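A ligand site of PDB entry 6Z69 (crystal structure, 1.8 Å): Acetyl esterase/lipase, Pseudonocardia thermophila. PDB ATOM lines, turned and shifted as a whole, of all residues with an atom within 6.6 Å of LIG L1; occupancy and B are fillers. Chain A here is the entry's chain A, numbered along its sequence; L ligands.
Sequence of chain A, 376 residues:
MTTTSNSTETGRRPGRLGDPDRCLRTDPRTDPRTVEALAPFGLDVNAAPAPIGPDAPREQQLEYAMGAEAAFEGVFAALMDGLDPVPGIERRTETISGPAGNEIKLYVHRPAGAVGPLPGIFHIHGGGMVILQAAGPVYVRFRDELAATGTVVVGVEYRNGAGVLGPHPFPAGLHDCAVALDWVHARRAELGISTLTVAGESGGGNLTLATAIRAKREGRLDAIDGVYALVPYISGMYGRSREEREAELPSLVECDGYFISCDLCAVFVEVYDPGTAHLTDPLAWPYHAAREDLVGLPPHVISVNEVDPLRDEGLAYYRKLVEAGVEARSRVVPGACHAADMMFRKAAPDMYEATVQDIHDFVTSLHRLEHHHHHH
A phosphorus (P1) of LIG L1 is bonded to the side-chain hydroxyl of Ser 202. The backbone NH of Gly 128 is in hydrogen-bond range of an oxygen (O1) of LIG L1 (2.8 Å). The backbone NH (N) of Gly 203 is in hydrogen-bond range of an oxygen (O1) of LIG L1, 2.8 Å away. N of Gly 127 lies within hydrogen-bond range of O1 of LIG L1 (2.8 Å). An oxygen (O1) of LG2 L2 is in hydrogen-bond range of the backbone NH (N) of Gly 128 (2.8 Å).
O of Ser 202 sits at hydrogen-bond distance from N of Tyr 233, 3.2 Å away. OG of Ser 202 lies within hydrogen-bond range of NE2 of His 338, at 3.0 Å. The backbone NH (N) of Ser 202 lies close to the backbone carbonyl oxygen (O) of Val 231. OE2 of Glu 201 sits at hydrogen-bond distance from OH of Tyr 139, at 2.6 Å. The side-chain carboxylate of Glu 201 is in hydrogen-bond range of the backbone NH of Gly 126 (2.9 Å). The side-chain hydroxyl of Tyr 139 lies within hydrogen-bond range of the backbone NH of Gly 126 (3.3 Å).
Merely in contact with LIG L1: Tyr 233 (2.8 Å), His 338 (3.2 Å), Glu 201 (3.5 Å), Tyr 139 (3.5 Å), Ala 339 (3.6 Å), Gly 126 (3.8 Å), Phe 76 (3.8 Å) and Met 343 (3.9 Å). Of the 25 residues printed, 12 come within 4 Å of LIG L1. The nearest printed residue that does not touch LIG L1 is Val 138 (4.05 Å).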
ATOM      1  N   PHE A  76     -14.111 -19.258  12.632  1.00  0.00           N
ATOM      2  CA  PHE A  76     -14.918 -20.464  12.300  1.00  0.00           C
ATOM      3  C   PHE A  76     -16.340 -20.283  12.798  1.00  0.00           C
ATOM      4  O   PHE A  76     -17.287 -20.613  12.032  1.00  0.00           O
ATOM      5  CB  PHE A  76     -14.234 -21.718  12.835  1.00  0.00           C
ATOM      6  CG  PHE A  76     -12.900 -21.968  12.179  1.00  0.00           C
ATOM      7  CD1 PHE A  76     -12.647 -21.532  10.887  1.00  0.00           C
ATOM      8  CD2 PHE A  76     -11.880 -22.558  12.882  1.00  0.00           C
ATOM      9  CE1 PHE A  76     -11.431 -21.761  10.273  1.00  0.00           C
ATOM     10  CE2 PHE A  76     -10.644 -22.744  12.287  1.00  0.00           C
ATOM     11  CZ  PHE A  76     -10.432 -22.353  10.988  1.00  0.00           C
ATOM     12  N   HIS A 125     -10.706 -34.130  13.782  1.00  0.00           N
ATOM     13  CA  HIS A 125     -10.682 -32.703  13.399  1.00  0.00           C
ATOM     14  C   HIS A 125      -9.247 -32.233  13.121  1.00  0.00           C
ATOM     15  O   HIS A 125      -8.280 -32.797  13.707  1.00  0.00           O
ATOM     16  CB  HIS A 125     -11.366 -31.837  14.459  1.00  0.00           C
ATOM     17  CG  HIS A 125     -10.570 -31.742  15.724  1.00  0.00           C
ATOM     18  ND1 HIS A 125      -9.553 -30.861  15.859  1.00  0.00           N
ATOM     19  CD2 HIS A 125     -10.598 -32.477  16.853  1.00  0.00           C
ATOM     20  CE1 HIS A 125      -8.989 -31.001  17.042  1.00  0.00           C
ATOM     21  NE2 HIS A 125      -9.667 -31.934  17.707  1.00  0.00           N
ATOM     22  N   GLY A 126      -9.135 -31.168  12.360  1.00  0.00           N
ATOM     23  CA  GLY A 126      -7.876 -30.465  12.096  1.00  0.00           C
ATOM     24  C   GLY A 126      -7.524 -29.402  13.135  1.00  0.00           C
ATOM     25  O   GLY A 126      -8.210 -29.271  14.194  1.00  0.00           O
ATOM     26  N   GLY A 127      -6.461 -28.683  12.850  1.00  0.00           N
ATOM     27  CA  GLY A 127      -5.799 -27.749  13.786  1.00  0.00           C
ATOM     28  C   GLY A 127      -4.374 -28.164  14.049  1.00  0.00           C
ATOM     29  O   GLY A 127      -3.876 -27.913  15.157  1.00  0.00           O
ATOM     30  N   GLY A 128      -3.709 -28.761  13.065  1.00  0.00           N
ATOM     31  CA  GLY A 128      -2.247 -29.047  13.128  1.00  0.00           C
ATOM     32  C   GLY A 128      -1.860 -29.943  14.286  1.00  0.00           C
ATOM     33  O   GLY A 128      -0.676 -29.925  14.680  1.00  0.00           O
ATOM     34  N   MET A 129      -2.801 -30.756  14.792  1.00  0.00           N
ATOM     35  CA  MET A 129      -2.676 -31.638  15.989  1.00  0.00           C
ATOM     36  C   MET A 129      -2.361 -30.832  17.249  1.00  0.00           C
ATOM     37  O   MET A 129      -2.090 -31.468  18.308  1.00  0.00           O
ATOM     38  CB  MET A 129      -1.613 -32.710  15.768  1.00  0.00           C
ATOM     39  CG  MET A 129      -1.893 -33.558  14.539  1.00  0.00           C
ATOM     40  SD  MET A 129      -1.173 -32.979  12.970  1.00  0.00           S
ATOM     41  CE  MET A 129       0.578 -33.125  13.312  1.00  0.00           C
ATOM     42  N   LEU A 132      -7.718 -26.203  18.284  1.00  0.00           N
ATOM     43  CA  LEU A 132      -9.130 -26.271  17.827  1.00  0.00           C
ATOM     44  C   LEU A 132      -9.821 -27.464  18.512  1.00  0.00           C
ATOM     45  O   LEU A 132      -9.143 -28.457  18.815  1.00  0.00           O
ATOM     46  CB  LEU A 132      -9.238 -26.430  16.299  1.00  0.00           C
ATOM     47  CG  LEU A 132      -8.594 -25.328  15.456  1.00  0.00           C
ATOM     48  CD1 LEU A 132      -8.762 -25.637  13.947  1.00  0.00           C
ATOM     49  CD2 LEU A 132      -9.110 -23.938  15.832  1.00  0.00           C
ATOM     50  N   VAL A 138     -17.557 -25.404  13.280  1.00  0.00           N
ATOM     51  CA  VAL A 138     -17.108 -25.894  11.951  1.00  0.00           C
ATOM     52  C   VAL A 138     -17.192 -27.446  11.929  1.00  0.00           C
ATOM     53  O   VAL A 138     -17.599 -28.024  10.909  1.00  0.00           O
ATOM     54  CB  VAL A 138     -15.739 -25.320  11.536  1.00  0.00           C
ATOM     55  CG1 VAL A 138     -14.555 -25.905  12.290  1.00  0.00           C
ATOM     56  CG2 VAL A 138     -15.490 -25.470  10.060  1.00  0.00           C
ATOM     57  N   TYR A 139     -16.813 -28.125  13.006  1.00  0.00           N
ATOM     58  CA  TYR A 139     -16.744 -29.612  13.075  1.00  0.00           C
ATOM     59  C   TYR A 139     -18.124 -30.159  13.407  1.00  0.00           C
ATOM     60  O   TYR A 139     -18.534 -31.203  12.838  1.00  0.00           O
ATOM     61  CB  TYR A 139     -15.613 -30.066  14.014  1.00  0.00           C
ATOM     62  CG  TYR A 139     -14.272 -29.617  13.505  1.00  0.00           C
ATOM     63  CD1 TYR A 139     -13.785 -30.083  12.297  1.00  0.00           C
ATOM     64  CD2 TYR A 139     -13.553 -28.620  14.157  1.00  0.00           C
ATOM     65  CE1 TYR A 139     -12.585 -29.648  11.777  1.00  0.00           C
ATOM     66  CE2 TYR A 139     -12.315 -28.198  13.669  1.00  0.00           C
ATOM     67  CZ  TYR A 139     -11.844 -28.696  12.462  1.00  0.00           C
ATOM     68  OH  TYR A 139     -10.650 -28.268  11.946  1.00  0.00           O
ATOM     69  N   GLU A 201      -9.415 -33.837   8.085  1.00  0.00           N
ATOM     70  CA  GLU A 201      -8.725 -32.834   7.233  1.00  0.00           C
ATOM     71  C   GLU A 201      -7.502 -32.269   7.950  1.00  0.00           C
ATOM     72  O   GLU A 201      -7.546 -32.047   9.200  1.00  0.00           O
ATOM     73  CB  GLU A 201      -9.701 -31.728   6.841  1.00  0.00           C
ATOM     74  CG  GLU A 201      -9.720 -30.507   7.737  1.00  0.00           C
ATOM     75  CD  GLU A 201     -10.232 -30.653   9.156  1.00  0.00           C
ATOM     76  OE1 GLU A 201     -10.867 -31.655   9.477  1.00  0.00           O
ATOM     77  OE2 GLU A 201      -9.907 -29.756   9.946  1.00  0.00           O
ATOM     78  N   SER A 202      -6.486 -31.960   7.156  1.00  0.00           N
ATOM     79  CA  SER A 202      -5.299 -31.166   7.582  1.00  0.00           C
ATOM     80  C   SER A 202      -4.638 -31.945   8.704  1.00  0.00           C
ATOM     81  O   SER A 202      -4.342 -33.108   8.466  1.00  0.00           O
ATOM     82  CB  SER A 202      -5.726 -29.750   7.920  1.00  0.00           C
ATOM     83  OG  SER A 202      -4.614 -28.885   8.114  1.00  0.00           O
ATOM     84  N   GLY A 203      -4.531 -31.389   9.915  1.00  0.00           N
ATOM     85  CA  GLY A 203      -3.974 -32.146  11.056  1.00  0.00           C
ATOM     86  C   GLY A 203      -4.769 -33.418  11.340  1.00  0.00           C
ATOM     87  O   GLY A 203      -4.191 -34.387  11.797  1.00  0.00           O
ATOM     88  N   GLY A 204      -6.063 -33.395  11.109  1.00  0.00           N
ATOM     89  CA  GLY A 204      -6.961 -34.563  11.292  1.00  0.00           C
ATOM     90  C   GLY A 204      -6.716 -35.587  10.194  1.00  0.00           C
ATOM     91  O   GLY A 204      -6.930 -36.814  10.426  1.00  0.00           O
ATOM     92  N   VAL A 231      -7.013 -32.793   2.495  1.00  0.00           N
ATOM     93  CA  VAL A 231      -5.945 -31.749   2.596  1.00  0.00           C
ATOM     94  C   VAL A 231      -4.971 -32.137   3.710  1.00  0.00           C
ATOM     95  O   VAL A 231      -4.737 -31.387   4.650  1.00  0.00           O
ATOM     96  CB  VAL A 231      -6.588 -30.361   2.786  1.00  0.00           C
ATOM     97  CG1 VAL A 231      -7.381 -29.979   1.543  1.00  0.00           C
ATOM     98  CG2 VAL A 231      -7.500 -30.261   4.015  1.00  0.00           C
ATOM     99  N   TYR A 233      -2.044 -32.741   6.289  1.00  0.00           N
ATOM    100  CA  TYR A 233      -0.914 -31.960   6.855  1.00  0.00           C
ATOM    101  C   TYR A 233       0.140 -32.944   7.340  1.00  0.00           C
ATOM    102  O   TYR A 233       0.092 -33.313   8.522  1.00  0.00           O
ATOM    103  CB  TYR A 233      -1.489 -31.064   7.948  1.00  0.00           C
ATOM    104  CG  TYR A 233      -0.518 -30.291   8.799  1.00  0.00           C
ATOM    105  CD1 TYR A 233       0.140 -29.171   8.330  1.00  0.00           C
ATOM    106  CD2 TYR A 233      -0.358 -30.630  10.141  1.00  0.00           C
ATOM    107  CE1 TYR A 233       0.998 -28.447   9.139  1.00  0.00           C
ATOM    108  CE2 TYR A 233       0.492 -29.906  10.962  1.00  0.00           C
ATOM    109  CZ  TYR A 233       1.144 -28.789  10.481  1.00  0.00           C
ATOM    110  OH  TYR A 233       1.954 -28.085  11.328  1.00  0.00           O
ATOM    111  N   TYR A 238       7.685 -27.602   6.852  1.00  0.00           N
ATOM    112  CA  TYR A 238       7.273 -26.199   6.651  1.00  0.00           C
ATOM    113  C   TYR A 238       8.446 -25.281   7.014  1.00  0.00           C
ATOM    114  O   TYR A 238       8.479 -24.189   6.436  1.00  0.00           O
ATOM    115  CB  TYR A 238       5.951 -25.942   7.414  1.00  0.00           C
ATOM    116  CG  TYR A 238       5.014 -27.116   7.250  1.00  0.00           C
ATOM    117  CD1 TYR A 238       4.536 -27.480   6.002  1.00  0.00           C
ATOM    118  CD2 TYR A 238       4.732 -27.958   8.311  1.00  0.00           C
ATOM    119  CE1 TYR A 238       3.780 -28.619   5.823  1.00  0.00           C
ATOM    120  CE2 TYR A 238       3.970 -29.107   8.153  1.00  0.00           C
ATOM    121  CZ  TYR A 238       3.487 -29.437   6.900  1.00  0.00           C
ATOM    122  OH  TYR A 238       2.825 -30.622   6.739  1.00  0.00           O
ATOM    123  N   PHE A 259      -4.178 -18.719   3.169  1.00  0.00           N
ATOM    124  CA  PHE A 259      -4.921 -19.141   4.393  1.00  0.00           C
ATOM    125  C   PHE A 259      -3.948 -19.647   5.478  1.00  0.00           C
ATOM    126  O   PHE A 259      -4.020 -19.212   6.676  1.00  0.00           O
ATOM    127  CB  PHE A 259      -6.000 -20.189   4.085  1.00  0.00           C
ATOM    128  CG  PHE A 259      -6.863 -20.456   5.295  1.00  0.00           C
ATOM    129  CD1 PHE A 259      -7.731 -19.487   5.756  1.00  0.00           C
ATOM    130  CD2 PHE A 259      -6.752 -21.640   5.998  1.00  0.00           C
ATOM    131  CE1 PHE A 259      -8.488 -19.698   6.904  1.00  0.00           C
ATOM    132  CE2 PHE A 259      -7.489 -21.846   7.158  1.00  0.00           C
ATOM    133  CZ  PHE A 259      -8.348 -20.884   7.600  1.00  0.00           C
ATOM    134  N   ILE A 260      -3.066 -20.580   5.124  1.00  0.00           N
ATOM    135  CA  ILE A 260      -2.017 -21.101   6.057  1.00  0.00           C
ATOM    136  C   ILE A 260      -0.624 -20.743   5.558  1.00  0.00           C
ATOM    137  O   ILE A 260      -0.422 -20.595   4.306  1.00  0.00           O
ATOM    138  CB  ILE A 260      -2.197 -22.608   6.322  1.00  0.00           C
ATOM    139  CG1 ILE A 260      -2.112 -23.447   5.051  1.00  0.00           C
ATOM    140  CG2 ILE A 260      -3.491 -22.891   7.127  1.00  0.00           C
ATOM    141  CD1 ILE A 260      -1.862 -24.913   5.338  1.00  0.00           C
ATOM    142  N   CYS A 265       3.213 -22.858  10.600  1.00  0.00           N
ATOM    143  CA  CYS A 265       3.174 -24.341  10.660  1.00  0.00           C
ATOM    144  C   CYS A 265       4.505 -24.813  11.250  1.00  0.00           C
ATOM    145  O   CYS A 265       4.507 -25.745  12.057  1.00  0.00           O
ATOM    146  CB  CYS A 265       2.907 -24.964   9.305  1.00  0.00           C
ATOM    147  SG  CYS A 265       1.223 -24.649   8.705  1.00  0.00           S
ATOM    148  N   PHE A 268       4.283 -24.810  14.750  1.00  0.00           N
ATOM    149  CA  PHE A 268       3.302 -25.807  15.256  1.00  0.00           C
ATOM    150  C   PHE A 268       3.938 -27.207  15.187  1.00  0.00           C
ATOM    151  O   PHE A 268       3.573 -28.091  15.983  1.00  0.00           O
ATOM    152  CB  PHE A 268       1.987 -25.712  14.470  1.00  0.00           C
ATOM    153  CG  PHE A 268       1.068 -24.563  14.808  1.00  0.00           C
ATOM    154  CD1 PHE A 268       1.358 -23.682  15.842  1.00  0.00           C
ATOM    155  CD2 PHE A 268      -0.066 -24.349  14.052  1.00  0.00           C
ATOM    156  CE1 PHE A 268       0.501 -22.638  16.124  1.00  0.00           C
ATOM    157  CE2 PHE A 268      -0.931 -23.304  14.346  1.00  0.00           C
ATOM    158  CZ  PHE A 268      -0.623 -22.445  15.376  1.00  0.00           C
ATOM    159  N   LEU A 310      -0.360 -27.421   1.010  1.00  0.00           N
ATOM    160  CA  LEU A 310      -0.242 -28.878   1.307  1.00  0.00           C
ATOM    161  C   LEU A 310      -0.580 -29.759   0.086  1.00  0.00           C
ATOM    162  O   LEU A 310      -0.492 -30.984   0.229  1.00  0.00           O
ATOM    163  CB  LEU A 310      -1.134 -29.224   2.503  1.00  0.00           C
ATOM    164  CG  LEU A 310      -0.931 -28.347   3.733  1.00  0.00           C
ATOM    165  CD1 LEU A 310      -1.886 -28.742   4.825  1.00  0.00           C
ATOM    166  CD2 LEU A 310       0.520 -28.389   4.243  1.00  0.00           C
ATOM    167  N   HIS A 338      -6.729 -24.162   1.138  1.00  0.00           N
ATOM    168  CA  HIS A 338      -6.751 -25.174   2.225  1.00  0.00           C
ATOM    169  C   HIS A 338      -8.124 -25.202   2.928  1.00  0.00           C
ATOM    170  O   HIS A 338      -8.578 -24.137   3.398  1.00  0.00           O
ATOM    171  CB  HIS A 338      -5.664 -24.879   3.227  1.00  0.00           C
ATOM    172  CG  HIS A 338      -5.638 -25.929   4.288  1.00  0.00           C
ATOM    173  ND1 HIS A 338      -5.157 -27.202   4.018  1.00  0.00           N
ATOM    174  CD2 HIS A 338      -6.217 -25.968   5.511  1.00  0.00           C
ATOM    175  CE1 HIS A 338      -5.355 -27.949   5.101  1.00  0.00           C
ATOM    176  NE2 HIS A 338      -5.978 -27.222   6.039  1.00  0.00           N
ATOM    177  N   ALA A 339      -8.761 -26.382   2.973  1.00  0.00           N
ATOM    178  CA  ALA A 339     -10.009 -26.676   3.698  1.00  0.00           C
ATOM    179  C   ALA A 339     -11.172 -25.811   3.211  1.00  0.00           C
ATOM    180  O   ALA A 339     -12.189 -25.739   3.937  1.00  0.00           O
ATOM    181  CB  ALA A 339      -9.787 -26.514   5.189  1.00  0.00           C
ATOM    182  N   MET A 342     -14.593 -27.213   3.443  1.00  0.00           N
ATOM    183  CA  MET A 342     -15.220 -27.435   4.761  1.00  0.00           C
ATOM    184  C   MET A 342     -15.483 -26.122   5.487  1.00  0.00           C
ATOM    185  O   MET A 342     -16.269 -26.155   6.434  1.00  0.00           O
ATOM    186  CB  MET A 342     -14.345 -28.359   5.614  1.00  0.00           C
ATOM    187  CG  MET A 342     -14.396 -29.778   5.058  1.00  0.00           C
ATOM    188  SD  MET A 342     -13.102 -30.878   5.762  1.00  0.00           S
ATOM    189  CE  MET A 342     -13.233 -30.167   7.409  1.00  0.00           C
ATOM    190  N   MET A 343     -14.882 -25.001   5.049  1.00  0.00           N
ATOM    191  CA  MET A 343     -15.086 -23.688   5.702  1.00  0.00           C
ATOM    192  C   MET A 343     -16.259 -22.927   5.089  1.00  0.00           C
ATOM    193  O   MET A 343     -16.942 -22.253   5.859  1.00  0.00           O
ATOM    194  CB  MET A 343     -13.829 -22.818   5.653  1.00  0.00           C
ATOM    195  CG  MET A 343     -12.688 -23.446   6.440  1.00  0.00           C
ATOM    196  SD  MET A 343     -11.323 -22.305   6.653  1.00  0.00           S
ATOM    197  CE  MET A 343     -10.705 -22.210   4.969  1.00  0.00           C
HETATM  198  C1  LIG L   1      -5.606 -26.515   9.091  1.00  0.00           C
HETATM  199  C2  LIG L   1      -7.076 -26.780   9.239  1.00  0.00           C
HETATM  200  C3  LIG L   1      -7.859 -25.487   9.314  1.00  0.00           C
HETATM  201  C4  LIG L   1      -9.268 -25.794   9.817  1.00  0.00           C
HETATM  202  C5  LIG L   1     -10.145 -26.474   8.770  1.00  0.00           C
HETATM  203  C6  LIG L   1     -11.630 -26.163   9.065  1.00  0.00           C
HETATM  204  P1  LIG L   1      -4.574 -27.937   9.291  1.00  0.00           P
HETATM  205  O1  LIG L   1      -4.840 -28.712  10.542  1.00  0.00           O
HETATM  206  O2  LIG L   1      -3.216 -27.073   9.280  1.00  0.00           O
HETATM  207  C7  LIG L   1      -2.013 -27.636   9.255  1.00  0.00           C
HETATM  208  C1  LG2 L   2      -4.126 -20.980  10.394  1.00  0.00           C
HETATM  209  C2  LG2 L   2      -3.022 -20.356   9.790  1.00  0.00           C
HETATM  210  C3  LG2 L   2      -1.742 -21.037   9.751  1.00  0.00           C
HETATM  211  C4  LG2 L   2      -3.606 -24.807  12.076  1.00  0.00           C
HETATM  212  C5  LG2 L   2      -4.959 -24.201  12.172  1.00  0.00           C
HETATM  213  C6  LG2 L   2      -5.089 -22.958  11.604  1.00  0.00           C
HETATM  214  O1  LG2 L   2      -3.389 -26.049  12.589  1.00  0.00           O
HETATM  215  O2  LG2 L   2      -2.564 -24.192  11.441  1.00  0.00           O
HETATM  216  C7  LG2 L   2      -6.463 -22.317  11.678  1.00  0.00           C
HETATM  217  C8  LG2 L   2      -4.014 -22.292  10.996  1.00  0.00           C
HETATM  218  C9  LG2 L   2      -2.704 -22.935  10.900  1.00  0.00           C
HETATM  219  C10 LG2 L   2      -1.634 -22.361  10.309  1.00  0.00           C
HETATM  220  O3  LG2 L   2      -0.673 -20.373   9.131  1.00  0.00           O
